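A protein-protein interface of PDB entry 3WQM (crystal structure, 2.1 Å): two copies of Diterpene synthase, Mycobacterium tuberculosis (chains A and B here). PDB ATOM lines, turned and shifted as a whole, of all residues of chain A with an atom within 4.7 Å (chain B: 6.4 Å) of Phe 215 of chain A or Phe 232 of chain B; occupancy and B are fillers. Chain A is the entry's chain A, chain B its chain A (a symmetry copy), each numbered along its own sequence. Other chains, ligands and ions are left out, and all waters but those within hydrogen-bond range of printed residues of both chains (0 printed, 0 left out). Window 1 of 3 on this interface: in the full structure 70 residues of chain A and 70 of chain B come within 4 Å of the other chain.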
ATOM      1  N   GLY A 213       7.986 -24.966 -29.115  1.00  0.00           N
ATOM      2  CA  GLY A 213       8.109 -26.218 -28.395  1.00  0.00           C
ATOM      3  C   GLY A 213       6.759 -26.817 -28.060  1.00  0.00           C
ATOM      4  O   GLY A 213       5.871 -26.913 -28.913  1.00  0.00           O
ATOM      5  N   ARG A 214       6.609 -27.219 -26.804  1.00  0.00           N
ATOM      6  CA  ARG A 214       5.372 -27.820 -26.330  1.00  0.00           C
ATOM      7  C   ARG A 214       4.169 -26.929 -26.626  1.00  0.00           C
ATOM      8  O   ARG A 214       4.201 -25.727 -26.362  1.00  0.00           O
ATOM      9  CB  ARG A 214       5.481 -28.091 -24.825  1.00  0.00           C
ATOM     10  CG  ARG A 214       6.407 -29.256 -24.495  1.00  0.00           C
ATOM     11  CD  ARG A 214       6.721 -29.321 -23.005  1.00  0.00           C
ATOM     12  NE  ARG A 214       7.533 -28.176 -22.604  1.00  0.00           N
ATOM     13  CZ  ARG A 214       7.921 -27.929 -21.354  1.00  0.00           C
ATOM     14  NH1 ARG A 214       7.571 -28.750 -20.369  1.00  0.00           N
ATOM     15  NH2 ARG A 214       8.658 -26.858 -21.088  1.00  0.00           N
ATOM     16  N   PHE A 215       3.121 -27.521 -27.197  1.00  0.00           N
ATOM     17  CA  PHE A 215       1.915 -26.761 -27.520  1.00  0.00           C
ATOM     18  C   PHE A 215       1.243 -26.358 -26.205  1.00  0.00           C
ATOM     19  O   PHE A 215       0.747 -27.201 -25.466  1.00  0.00           O
ATOM     20  CB  PHE A 215       0.927 -27.603 -28.355  1.00  0.00           C
ATOM     21  CG  PHE A 215       1.398 -27.928 -29.763  1.00  0.00           C
ATOM     22  CD1 PHE A 215       2.730 -27.739 -30.154  1.00  0.00           C
ATOM     23  CD2 PHE A 215       0.500 -28.474 -30.690  1.00  0.00           C
ATOM     24  CE1 PHE A 215       3.171 -28.094 -31.450  1.00  0.00           C
ATOM     25  CE2 PHE A 215       0.922 -28.832 -31.986  1.00  0.00           C
ATOM     26  CZ  PHE A 215       2.271 -28.642 -32.366  1.00  0.00           C
ATOM     27  N   SER A 216       1.233 -25.065 -25.919  1.00  0.00           N
ATOM     28  CA  SER A 216       0.610 -24.564 -24.699  1.00  0.00           C
ATOM     29  C   SER A 216       0.574 -23.052 -24.792  1.00  0.00           C
ATOM     30  O   SER A 216       1.379 -22.460 -25.502  1.00  0.00           O
ATOM     31  CB  SER A 216       1.428 -24.968 -23.473  1.00  0.00           C
ATOM     32  OG  SER A 216       2.630 -24.235 -23.441  1.00  0.00           O
ATOM     33  N   LEU A 230      -3.410 -19.966 -32.869  1.00  0.00           N
ATOM     34  CA  LEU A 230      -2.213 -20.475 -32.207  1.00  0.00           C
ATOM     35  C   LEU A 230      -1.158 -21.040 -33.140  1.00  0.00           C
ATOM     36  O   LEU A 230      -1.472 -21.783 -34.073  1.00  0.00           O
ATOM     37  CB  LEU A 230      -2.590 -21.559 -31.195  1.00  0.00           C
ATOM     38  CG  LEU A 230      -3.728 -21.149 -30.263  1.00  0.00           C
ATOM     39  CD1 LEU A 230      -4.015 -22.290 -29.312  1.00  0.00           C
ATOM     40  CD2 LEU A 230      -3.358 -19.858 -29.508  1.00  0.00           C
ATOM     41  N   PHE A 232       3.132 -22.574 -33.048  1.00  0.00           N
ATOM     42  CA  PHE A 232       4.234 -23.056 -32.235  1.00  0.00           C
ATOM     43  C   PHE A 232       5.431 -23.326 -33.125  1.00  0.00           C
ATOM     44  O   PHE A 232       5.393 -24.223 -33.960  1.00  0.00           O
ATOM     45  CB  PHE A 232       3.819 -24.331 -31.495  1.00  0.00           C
ATOM     46  CG  PHE A 232       2.570 -24.163 -30.676  1.00  0.00           C
ATOM     47  CD1 PHE A 232       2.593 -23.413 -29.502  1.00  0.00           C
ATOM     48  CD2 PHE A 232       1.351 -24.685 -31.121  1.00  0.00           C
ATOM     49  CE1 PHE A 232       1.430 -23.175 -28.782  1.00  0.00           C
ATOM     50  CE2 PHE A 232       0.177 -24.455 -30.406  1.00  0.00           C
ATOM     51  CZ  PHE A 232       0.217 -23.694 -29.230  1.00  0.00           C
ATOM     52  N   VAL A 286      -2.385 -36.654 -35.163  1.00  0.00           N
ATOM     53  CA  VAL A 286      -2.608 -35.645 -34.140  1.00  0.00           C
ATOM     54  C   VAL A 286      -1.375 -34.775 -33.914  1.00  0.00           C
ATOM     55  O   VAL A 286      -0.277 -35.285 -33.720  1.00  0.00           O
ATOM     56  CB  VAL A 286      -3.031 -36.310 -32.798  1.00  0.00           C
ATOM     57  CG1 VAL A 286      -2.124 -37.487 -32.491  1.00  0.00           C
ATOM     58  CG2 VAL A 286      -2.995 -35.296 -31.661  1.00  0.00           C
ATOM     59  N   PHE A 287      -1.569 -33.459 -33.954  1.00  0.00           N
ATOM     60  CA  PHE A 287      -0.491 -32.511 -33.734  1.00  0.00           C
ATOM     61  C   PHE A 287      -0.428 -32.194 -32.242  1.00  0.00           C
ATOM     62  O   PHE A 287      -1.459 -31.943 -31.610  1.00  0.00           O
ATOM     63  CB  PHE A 287      -0.746 -31.235 -34.543  1.00  0.00           C
ATOM     64  CG  PHE A 287      -0.605 -31.430 -36.027  1.00  0.00           C
ATOM     65  CD1 PHE A 287       0.646 -31.365 -36.633  1.00  0.00           C
ATOM     66  CD2 PHE A 287      -1.710 -31.739 -36.812  1.00  0.00           C
ATOM     67  CE1 PHE A 287       0.794 -31.611 -38.007  1.00  0.00           C
ATOM     68  CE2 PHE A 287      -1.574 -31.991 -38.188  1.00  0.00           C
ATOM     69  CZ  PHE A 287      -0.324 -31.928 -38.782  1.00  0.00           C
ATOM     70  N   GLY A 288       0.781 -32.206 -31.684  1.00  0.00           N
ATOM     71  CA  GLY A 288       0.942 -31.949 -30.267  1.00  0.00           C
ATOM     72  C   GLY A 288       1.596 -33.108 -29.525  1.00  0.00           C
ATOM     73  O   GLY A 288       2.024 -32.946 -28.381  1.00  0.00           O
ATOM     74  N   TRP A 297      11.655 -31.500 -25.541  1.00  0.00           N
ATOM     75  CA  TRP A 297      10.509 -32.035 -26.269  1.00  0.00           C
ATOM     76  C   TRP A 297      10.409 -31.395 -27.657  1.00  0.00           C
ATOM     77  O   TRP A 297      10.596 -30.187 -27.803  1.00  0.00           O
ATOM     78  CB  TRP A 297       9.237 -31.738 -25.460  1.00  0.00           C
ATOM     79  CG  TRP A 297       7.962 -32.305 -26.004  1.00  0.00           C
ATOM     80  CD1 TRP A 297       7.331 -33.443 -25.596  1.00  0.00           C
ATOM     81  CD2 TRP A 297       7.117 -31.708 -26.994  1.00  0.00           C
ATOM     82  NE1 TRP A 297       6.131 -33.587 -26.263  1.00  0.00           N
ATOM     83  CE2 TRP A 297       5.979 -32.532 -27.126  1.00  0.00           C
ATOM     84  CE3 TRP A 297       7.209 -30.546 -27.779  1.00  0.00           C
ATOM     85  CZ2 TRP A 297       4.940 -32.236 -28.009  1.00  0.00           C
ATOM     86  CZ3 TRP A 297       6.176 -30.251 -28.657  1.00  0.00           C
ATOM     87  CH2 TRP A 297       5.053 -31.095 -28.764  1.00  0.00           C
ATOM     88  N   ALA A 299       7.854 -31.547 -31.247  1.00  0.00           N
ATOM     89  CA  ALA A 299       6.606 -32.039 -31.828  1.00  0.00           C
ATOM     90  C   ALA A 299       6.919 -32.932 -33.021  1.00  0.00           C
ATOM     91  O   ALA A 299       7.810 -32.617 -33.810  1.00  0.00           O
ATOM     92  CB  ALA A 299       5.748 -30.866 -32.288  1.00  0.00           C
ATOM     93  N   PHE B 209      -6.034 -30.174 -23.371  1.00  0.00           N
ATOM     94  CA  PHE B 209      -7.130 -29.743 -24.223  1.00  0.00           C
ATOM     95  C   PHE B 209      -6.914 -30.454 -25.555  1.00  0.00           C
ATOM     96  O   PHE B 209      -5.815 -30.392 -26.126  1.00  0.00           O
ATOM     97  CB  PHE B 209      -7.099 -28.216 -24.412  1.00  0.00           C
ATOM     98  CG  PHE B 209      -8.111 -27.694 -25.417  1.00  0.00           C
ATOM     99  CD1 PHE B 209      -7.904 -27.849 -26.787  1.00  0.00           C
ATOM    100  CD2 PHE B 209      -9.262 -27.042 -24.989  1.00  0.00           C
ATOM    101  CE1 PHE B 209      -8.826 -27.357 -27.715  1.00  0.00           C
ATOM    102  CE2 PHE B 209     -10.195 -26.546 -25.913  1.00  0.00           C
ATOM    103  CZ  PHE B 209      -9.973 -26.705 -27.277  1.00  0.00           C
ATOM    104  N   ILE B 210      -7.950 -31.144 -26.033  1.00  0.00           N
ATOM    105  CA  ILE B 210      -7.876 -31.856 -27.307  1.00  0.00           C
ATOM    106  C   ILE B 210      -8.859 -31.221 -28.280  1.00  0.00           C
ATOM    107  O   ILE B 210     -10.068 -31.379 -28.141  1.00  0.00           O
ATOM    108  CB  ILE B 210      -8.261 -33.346 -27.168  1.00  0.00           C
ATOM    109  CG1 ILE B 210      -7.352 -34.037 -26.143  1.00  0.00           C
ATOM    110  CG2 ILE B 210      -8.136 -34.045 -28.531  1.00  0.00           C
ATOM    111  CD1 ILE B 210      -7.834 -35.409 -25.745  1.00  0.00           C
ATOM    112  N   GLY B 211      -8.338 -30.485 -29.249  1.00  0.00           N
ATOM    113  CA  GLY B 211      -9.194 -29.860 -30.234  1.00  0.00           C
ATOM    114  C   GLY B 211      -8.940 -30.543 -31.559  1.00  0.00           C
ATOM    115  O   GLY B 211      -8.458 -31.672 -31.587  1.00  0.00           O
ATOM    116  N   PHE B 212      -9.247 -29.866 -32.659  1.00  0.00           N
ATOM    117  CA  PHE B 212      -9.020 -30.439 -33.979  1.00  0.00           C
ATOM    118  C   PHE B 212      -9.001 -29.311 -34.989  1.00  0.00           C
ATOM    119  O   PHE B 212      -9.536 -28.237 -34.731  1.00  0.00           O
ATOM    120  CB  PHE B 212     -10.116 -31.463 -34.324  1.00  0.00           C
ATOM    121  CG  PHE B 212     -11.378 -30.860 -34.881  1.00  0.00           C
ATOM    122  CD1 PHE B 212     -11.539 -30.698 -36.255  1.00  0.00           C
ATOM    123  CD2 PHE B 212     -12.413 -30.477 -34.037  1.00  0.00           C
ATOM    124  CE1 PHE B 212     -12.719 -30.164 -36.781  1.00  0.00           C
ATOM    125  CE2 PHE B 212     -13.600 -29.941 -34.553  1.00  0.00           C
ATOM    126  CZ  PHE B 212     -13.752 -29.785 -35.927  1.00  0.00           C
ATOM    127  N   GLY B 213      -8.371 -29.556 -36.129  1.00  0.00           N
ATOM    128  CA  GLY B 213      -8.293 -28.542 -37.162  1.00  0.00           C
ATOM    129  C   GLY B 213      -7.425 -27.373 -36.747  1.00  0.00           C
ATOM    130  O   GLY B 213      -6.307 -27.548 -36.252  1.00  0.00           O
ATOM    131  N   ARG B 214      -7.950 -26.170 -36.951  1.00  0.00           N
ATOM    132  CA  ARG B 214      -7.237 -24.949 -36.610  1.00  0.00           C
ATOM    133  C   ARG B 214      -6.778 -24.960 -35.155  1.00  0.00           C
ATOM    134  O   ARG B 214      -7.557 -25.277 -34.255  1.00  0.00           O
ATOM    135  CB  ARG B 214      -8.138 -23.741 -36.880  1.00  0.00           C
ATOM    136  CG  ARG B 214      -8.323 -23.454 -38.367  1.00  0.00           C
ATOM    137  CD  ARG B 214      -9.436 -22.443 -38.611  1.00  0.00           C
ATOM    138  NE  ARG B 214     -10.732 -23.015 -38.259  1.00  0.00           N
ATOM    139  CZ  ARG B 214     -11.887 -22.354 -38.315  1.00  0.00           C
ATOM    140  NH1 ARG B 214     -11.915 -21.086 -38.711  1.00  0.00           N
ATOM    141  NH2 ARG B 214     -13.016 -22.961 -37.970  1.00  0.00           N
ATOM    142  N   PHE B 215      -5.506 -24.633 -34.933  1.00  0.00           N
ATOM    143  CA  PHE B 215      -4.964 -24.607 -33.576  1.00  0.00           C
ATOM    144  C   PHE B 215      -5.617 -23.442 -32.828  1.00  0.00           C
ATOM    145  O   PHE B 215      -5.390 -22.281 -33.148  1.00  0.00           O
ATOM    146  CB  PHE B 215      -3.434 -24.407 -33.585  1.00  0.00           C
ATOM    147  CG  PHE B 215      -2.642 -25.578 -34.145  1.00  0.00           C
ATOM    148  CD1 PHE B 215      -3.262 -26.609 -34.862  1.00  0.00           C
ATOM    149  CD2 PHE B 215      -1.249 -25.616 -33.987  1.00  0.00           C
ATOM    150  CE1 PHE B 215      -2.509 -27.667 -35.423  1.00  0.00           C
ATOM    151  CE2 PHE B 215      -0.485 -26.663 -34.538  1.00  0.00           C
ATOM    152  CZ  PHE B 215      -1.123 -27.695 -35.265  1.00  0.00           C
ATOM    153  N   SER B 216      -6.430 -23.760 -31.833  1.00  0.00           N
ATOM    154  CA  SER B 216      -7.098 -22.733 -31.043  1.00  0.00           C
ATOM    155  C   SER B 216      -7.759 -23.420 -29.865  1.00  0.00           C
ATOM    156  O   SER B 216      -8.062 -24.605 -29.934  1.00  0.00           O
ATOM    157  CB  SER B 216      -8.170 -22.027 -31.873  1.00  0.00           C
ATOM    158  OG  SER B 216      -9.254 -22.900 -32.089  1.00  0.00           O
ATOM    159  N   THR B 217      -7.968 -22.676 -28.784  1.00  0.00           N
ATOM    160  CA  THR B 217      -8.603 -23.218 -27.592  1.00  0.00           C
ATOM    161  C   THR B 217      -9.712 -22.253 -27.213  1.00  0.00           C
ATOM    162  O   THR B 217      -9.667 -21.076 -27.567  1.00  0.00           O
ATOM    163  CB  THR B 217      -7.599 -23.365 -26.429  1.00  0.00           C
ATOM    164  OG1 THR B 217      -7.097 -22.079 -26.052  1.00  0.00           O
ATOM    165  CG2 THR B 217      -6.425 -24.236 -26.860  1.00  0.00           C
ATOM    166  N   GLY B 226      -0.213 -22.720 -18.259  1.00  0.00           N
ATOM    167  CA  GLY B 226       0.860 -23.067 -19.172  1.00  0.00           C
ATOM    168  C   GLY B 226       1.041 -24.576 -19.145  1.00  0.00           C
ATOM    169  O   GLY B 226       1.681 -25.152 -20.026  1.00  0.00           O
ATOM    170  N   THR B 228      -1.518 -26.689 -19.282  1.00  0.00           N
ATOM    171  CA  THR B 228      -2.612 -27.350 -19.987  1.00  0.00           C
ATOM    172  C   THR B 228      -2.000 -27.799 -21.327  1.00  0.00           C
ATOM    173  O   THR B 228      -1.772 -26.982 -22.210  1.00  0.00           O
ATOM    174  CB  THR B 228      -3.800 -26.379 -20.271  1.00  0.00           C
ATOM    175  OG1 THR B 228      -4.315 -25.865 -19.036  1.00  0.00           O
ATOM    176  CG2 THR B 228      -4.922 -27.109 -21.001  1.00  0.00           C
ATOM    177  N   SER B 229      -1.711 -29.089 -21.469  1.00  0.00           N
ATOM    178  CA  SER B 229      -1.121 -29.616 -22.712  1.00  0.00           C
ATOM    179  C   SER B 229      -2.125 -29.552 -23.870  1.00  0.00           C
ATOM    180  O   SER B 229      -3.228 -30.083 -23.767  1.00  0.00           O
ATOM    181  CB  SER B 229      -0.692 -31.078 -22.524  1.00  0.00           C
ATOM    182  OG  SER B 229       0.090 -31.257 -21.359  1.00  0.00           O
ATOM    183  N   LEU B 230      -1.728 -28.929 -24.974  1.00  0.00           N
ATOM    184  CA  LEU B 230      -2.607 -28.797 -26.132  1.00  0.00           C
ATOM    185  C   LEU B 230      -2.345 -29.791 -27.250  1.00  0.00           C
ATOM    186  O   LEU B 230      -1.194 -30.038 -27.619  1.00  0.00           O
ATOM    187  CB  LEU B 230      -2.506 -27.385 -26.712  1.00  0.00           C
ATOM    188  CG  LEU B 230      -2.643 -26.286 -25.660  1.00  0.00           C
ATOM    189  CD1 LEU B 230      -2.529 -24.941 -26.342  1.00  0.00           C
ATOM    190  CD2 LEU B 230      -3.981 -26.432 -24.910  1.00  0.00           C
ATOM    191  N   TYR B 231      -3.438 -30.335 -27.788  1.00  0.00           N
ATOM    192  CA  TYR B 231      -3.403 -31.296 -28.884  1.00  0.00           C
ATOM    193  C   TYR B 231      -4.479 -30.948 -29.920  1.00  0.00           C
ATOM    194  O   TYR B 231      -5.575 -30.481 -29.576  1.00  0.00           O
ATOM    195  CB  TYR B 231      -3.647 -32.708 -28.347  1.00  0.00           C
ATOM    196  CG  TYR B 231      -2.650 -33.122 -27.284  1.00  0.00           C
ATOM    197  CD1 TYR B 231      -1.404 -33.661 -27.632  1.00  0.00           C
ATOM    198  CD2 TYR B 231      -2.928 -32.920 -25.930  1.00  0.00           C
ATOM    199  CE1 TYR B 231      -0.461 -33.984 -26.650  1.00  0.00           C
ATOM    200  CE2 TYR B 231      -1.997 -33.235 -24.944  1.00  0.00           C
ATOM    201  CZ  TYR B 231      -0.769 -33.763 -25.305  1.00  0.00           C
ATOM    202  OH  TYR B 231       0.152 -34.042 -24.325  1.00  0.00           O
ATOM    203  N   PHE B 232      -4.164 -31.182 -31.189  1.00  0.00           N
ATOM    204  CA  PHE B 232      -5.098 -30.900 -32.264  1.00  0.00           C
ATOM    205  C   PHE B 232      -5.091 -32.054 -33.247  1.00  0.00           C
ATOM    206  O   PHE B 232      -4.090 -32.297 -33.912  1.00  0.00           O
ATOM    207  CB  PHE B 232      -4.706 -29.596 -32.968  1.00  0.00           C
ATOM    208  CG  PHE B 232      -4.586 -28.428 -32.029  1.00  0.00           C
ATOM    209  CD1 PHE B 232      -5.725 -27.857 -31.466  1.00  0.00           C
ATOM    210  CD2 PHE B 232      -3.329 -27.951 -31.643  1.00  0.00           C
ATOM    211  CE1 PHE B 232      -5.625 -26.836 -30.529  1.00  0.00           C
ATOM    212  CE2 PHE B 232      -3.216 -26.925 -30.707  1.00  0.00           C
ATOM    213  CZ  PHE B 232      -4.371 -26.365 -30.145  1.00  0.00           C
ATOM    214  N   THR B 233      -6.205 -32.780 -33.311  1.00  0.00           N
ATOM    215  CA  THR B 233      -6.330 -33.900 -34.237  1.00  0.00           C
ATOM    216  C   THR B 233      -6.662 -33.315 -35.608  1.00  0.00           C
ATOM    217  O   THR B 233      -7.089 -32.166 -35.716  1.00  0.00           O
ATOM    218  CB  THR B 233      -7.465 -34.868 -33.810  1.00  0.00           C
ATOM    219  OG1 THR B 233      -8.717 -34.171 -33.807  1.00  0.00           O
ATOM    220  CG2 THR B 233      -7.211 -35.412 -32.397  1.00  0.00           C
ATOM    221  N   VAL B 234      -6.438 -34.088 -36.661  1.00  0.00           N
ATOM    222  CA  VAL B 234      -6.749 -33.607 -37.995  1.00  0.00           C
ATOM    223  C   VAL B 234      -8.263 -33.674 -38.225  1.00  0.00           C
ATOM    224  O   VAL B 234      -8.864 -32.732 -38.743  1.00  0.00           O
ATOM    225  CB  VAL B 234      -6.020 -34.445 -39.063  1.00  0.00           C
ATOM    226  CG1 VAL B 234      -6.485 -34.037 -40.463  1.00  0.00           C
ATOM    227  CG2 VAL B 234      -4.520 -34.244 -38.926  1.00  0.00           C
ATOM    228  N   ILE B 248      -1.900 -39.455 -26.993  1.00  0.00           N
ATOM    229  CA  ILE B 248      -2.031 -38.132 -26.394  1.00  0.00           C
ATOM    230  C   ILE B 248      -1.778 -38.254 -24.888  1.00  0.00           C
ATOM    231  O   ILE B 248      -0.996 -37.493 -24.317  1.00  0.00           O
ATOM    232  CB  ILE B 248      -3.443 -37.551 -26.651  1.00  0.00           C
ATOM    233  CG1 ILE B 248      -3.556 -37.144 -28.124  1.00  0.00           C
ATOM    234  CG2 ILE B 248      -3.722 -36.374 -25.720  1.00  0.00           C
ATOM    235  CD1 ILE B 248      -4.944 -36.667 -28.545  1.00  0.00           C
ATOM    236  N   ARG B 256       5.666 -34.445 -21.921  1.00  0.00           N
ATOM    237  CA  ARG B 256       5.580 -32.998 -21.704  1.00  0.00           C
ATOM    238  C   ARG B 256       6.463 -32.525 -20.557  1.00  0.00           C
ATOM    239  O   ARG B 256       7.099 -31.475 -20.649  1.00  0.00           O
ATOM    240  CB  ARG B 256       4.131 -32.555 -21.467  1.00  0.00           C
ATOM    241  CG  ARG B 256       3.258 -32.581 -22.731  1.00  0.00           C
ATOM    242  CD  ARG B 256       3.885 -31.796 -23.898  1.00  0.00           C
ATOM    243  NE  ARG B 256       3.033 -31.793 -25.092  1.00  0.00           N
ATOM    244  CZ  ARG B 256       2.128 -30.854 -25.386  1.00  0.00           C
ATOM    245  NH1 ARG B 256       1.938 -29.820 -24.581  1.00  0.00           N
ATOM    246  NH2 ARG B 256       1.414 -30.946 -26.501  1.00  0.00           N
ATOM    247  N   PHE B 287       4.514 -25.005 -36.475  1.00  0.00           N
ATOM    248  CA  PHE B 287       3.276 -25.763 -36.446  1.00  0.00           C
ATOM    249  C   PHE B 287       2.120 -24.787 -36.237  1.00  0.00           C
ATOM    250  O   PHE B 287       2.193 -23.904 -35.377  1.00  0.00           O
ATOM    251  CB  PHE B 287       3.321 -26.791 -35.310  1.00  0.00           C
ATOM    252  CG  PHE B 287       4.291 -27.912 -35.557  1.00  0.00           C
ATOM    253  CD1 PHE B 287       3.918 -29.016 -36.317  1.00  0.00           C
ATOM    254  CD2 PHE B 287       5.597 -27.841 -35.083  1.00  0.00           C
ATOM    255  CE1 PHE B 287       4.839 -30.035 -36.608  1.00  0.00           C
ATOM    256  CE2 PHE B 287       6.529 -28.852 -35.370  1.00  0.00           C
ATOM    257  CZ  PHE B 287       6.149 -29.946 -36.131  1.00  0.00           C
ATOM    258  N   GLY B 288       1.059 -24.949 -37.024  1.00  0.00           N
ATOM    259  CA  GLY B 288      -0.076 -24.054 -36.924  1.00  0.00           C
ATOM    260  C   GLY B 288      -0.369 -23.321 -38.228  1.00  0.00           C
ATOM    261  O   GLY B 288      -1.437 -22.726 -38.375  1.00  0.00           O
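The backbone carbonyl oxygen (O) of Phe 209 of chain B lies within hydrogen-bond range of the backbone NH (N) of Tyr 231 of chain B (2.9 Å).
The backbone NH (N) of Gly 211 of chain B lies within hydrogen-bond range of the backbone carbonyl oxygen (O) of Tyr 231 of chain B, at 2.8 Å.
The backbone carbonyl oxygen (O) of Leu 230 of chain B is in hydrogen-bond range of the guanidinium group (NH2) of Arg 256 of chain B (3.0 Å).
The backbone carbonyl oxygen of Arg 256 of chain B is in hydrogen-bond range of the guanidinium group of Arg 214 of chain A.
N of Leu 230 of chain B lies within hydrogen-bond range of O of Phe 215 of chain A (3.1 Å).
NH1 of Arg 256 of chain B lies within hydrogen-bond range of O of Phe 215 of chain A (3.0 Å).
The backbone carbonyl oxygen (O) of Phe 215 of chain B is in hydrogen-bond range of the backbone NH (N) of Leu 230 of chain A.
O of Phe 232 of chain A is in hydrogen-bond range of N of Phe 287 of chain B (2.8 Å).
N of Phe 287 of chain A sits at hydrogen-bond distance from O of Phe 232 of chain B.
The guanidinium group (NH2) of Arg 256 of chain B sits at hydrogen-bond distance from the backbone carbonyl oxygen (O) of Gly 288 of chain A (2.8 Å).
Among the printed residues, pairs that only touch across the chains: Phe 215 of chain A with Phe 215 of chain B (3.6 Å), Phe 215 of chain A with Phe 232 of chain B (3.98 Å), Phe 215 of chain A with Phe 287 of chain B (3.6 Å), Ser 216 of chain A with Gly 226 of chain B (3.5 Å), Ser 216 of chain A with Thr 228 of chain B (3.99 Å), Ser 216 of chain A with Leu 230 of chain B (3.6 Å), Leu 230 of chain A with Ser 216 of chain B (3.6 Å), Leu 230 of chain A with Thr 217 of chain B (3.95 Å), Leu 230 of chain A with Gly 288 of chain B (3.9 Å), Phe 232 of chain A with Phe 215 of chain B (3.98 Å), Val 286 of chain A with Phe 232 of chain B (3.7 Å), Val 286 of chain A with Ile 248 of chain B (3.9 Å), Phe 287 of chain A with Phe 215 of chain B (3.6 Å), Phe 287 of chain A with Tyr 231 of chain B (3.4 Å), Phe 287 of chain A with Val 234 of chain B (3.8 Å), Gly 288 of chain A with Leu 230 of chain B (3.9 Å), Gly 288 of chain A with Tyr 231 of chain B (3.2 Å), Trp 297 of chain A with Arg 256 of chain B (3.5 Å) and Ala 299 of chain A with Phe 287 of chain B (3.8 Å).
Printed residues of chain B within 4 Å of Phe 215 of chain A: Phe 215 (3.6 Å), Leu 230 (3.1 Å), Phe 232 (3.98 Å), Arg 256 (3.0 Å) and Phe 287 (3.6 Å).
Of the printed residues of chain A, Phe 232 of chain B touches Phe 215 (3.98 Å), Val 286 (3.7 Å) and Phe 287 (2.8 Å).
Printed residues of chain A within 4 Å of Val 234 of chain B: Phe 287.
Printed residues of chain A within 4 Å of Arg 256 of chain B: Arg 214, Phe 215, Gly 288 and Trp 297.
Printed residues of chain B within 4 Å of Gly 288 of chain A: Leu 230 (3.9 Å), Tyr 231 (3.2 Å) and Arg 256 (2.8 Å).
Of the printed residues of chain A, Ile 248 of chain B touches Val 286.
Of the printed residues of chain A, Thr 228 of chain B touches Ser 216 (3.99 Å).
Ile 210 of chain B touches none of the printed residues of chain A.
The nearest printed residue of chain B that does not touch Phe 215 of chain A is Ser 229 of chain B (4.04 Å).
The nearest printed residue of chain A that does not touch Phe 232 of chain B is Leu 230 of chain A (4.2 Å).
Of the 11 printed residues of chain A, 10 touch a printed residue of chain B.
Hydrophobic or aromatic side chains of chain A within 4 Å of the printed part of chain B: Phe 215, Leu 230, Phe 232, Val 286, Phe 287, Trp 297 and Ala 299.
Hydrophobic or aromatic side chains of chain B that line the printed part of chain A: Phe 215, Leu 230, Tyr 231, Phe 232, Val 234, Ile 248 and Phe 287.
Phe 215 of chain A touches its own counterpart, Phe 215 of chain B.
Phe 215 of chain A touches Phe 287 of chain B, and with the chains exchanged Phe 287 of chain A touches Phe 215 of chain B.
Leu 230 of chain A touches Gly 288 of chain B, and with the chains exchanged Gly 288 of chain A touches Leu 230 of chain B.
Phe 232 of chain A touches Phe 287 of chain B, and with the chains exchanged Phe 287 of chain A touches Phe 232 of chain B.
Positions printed for both chains: 213, 214, 215, 216, 230, 232, 287 and 288.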
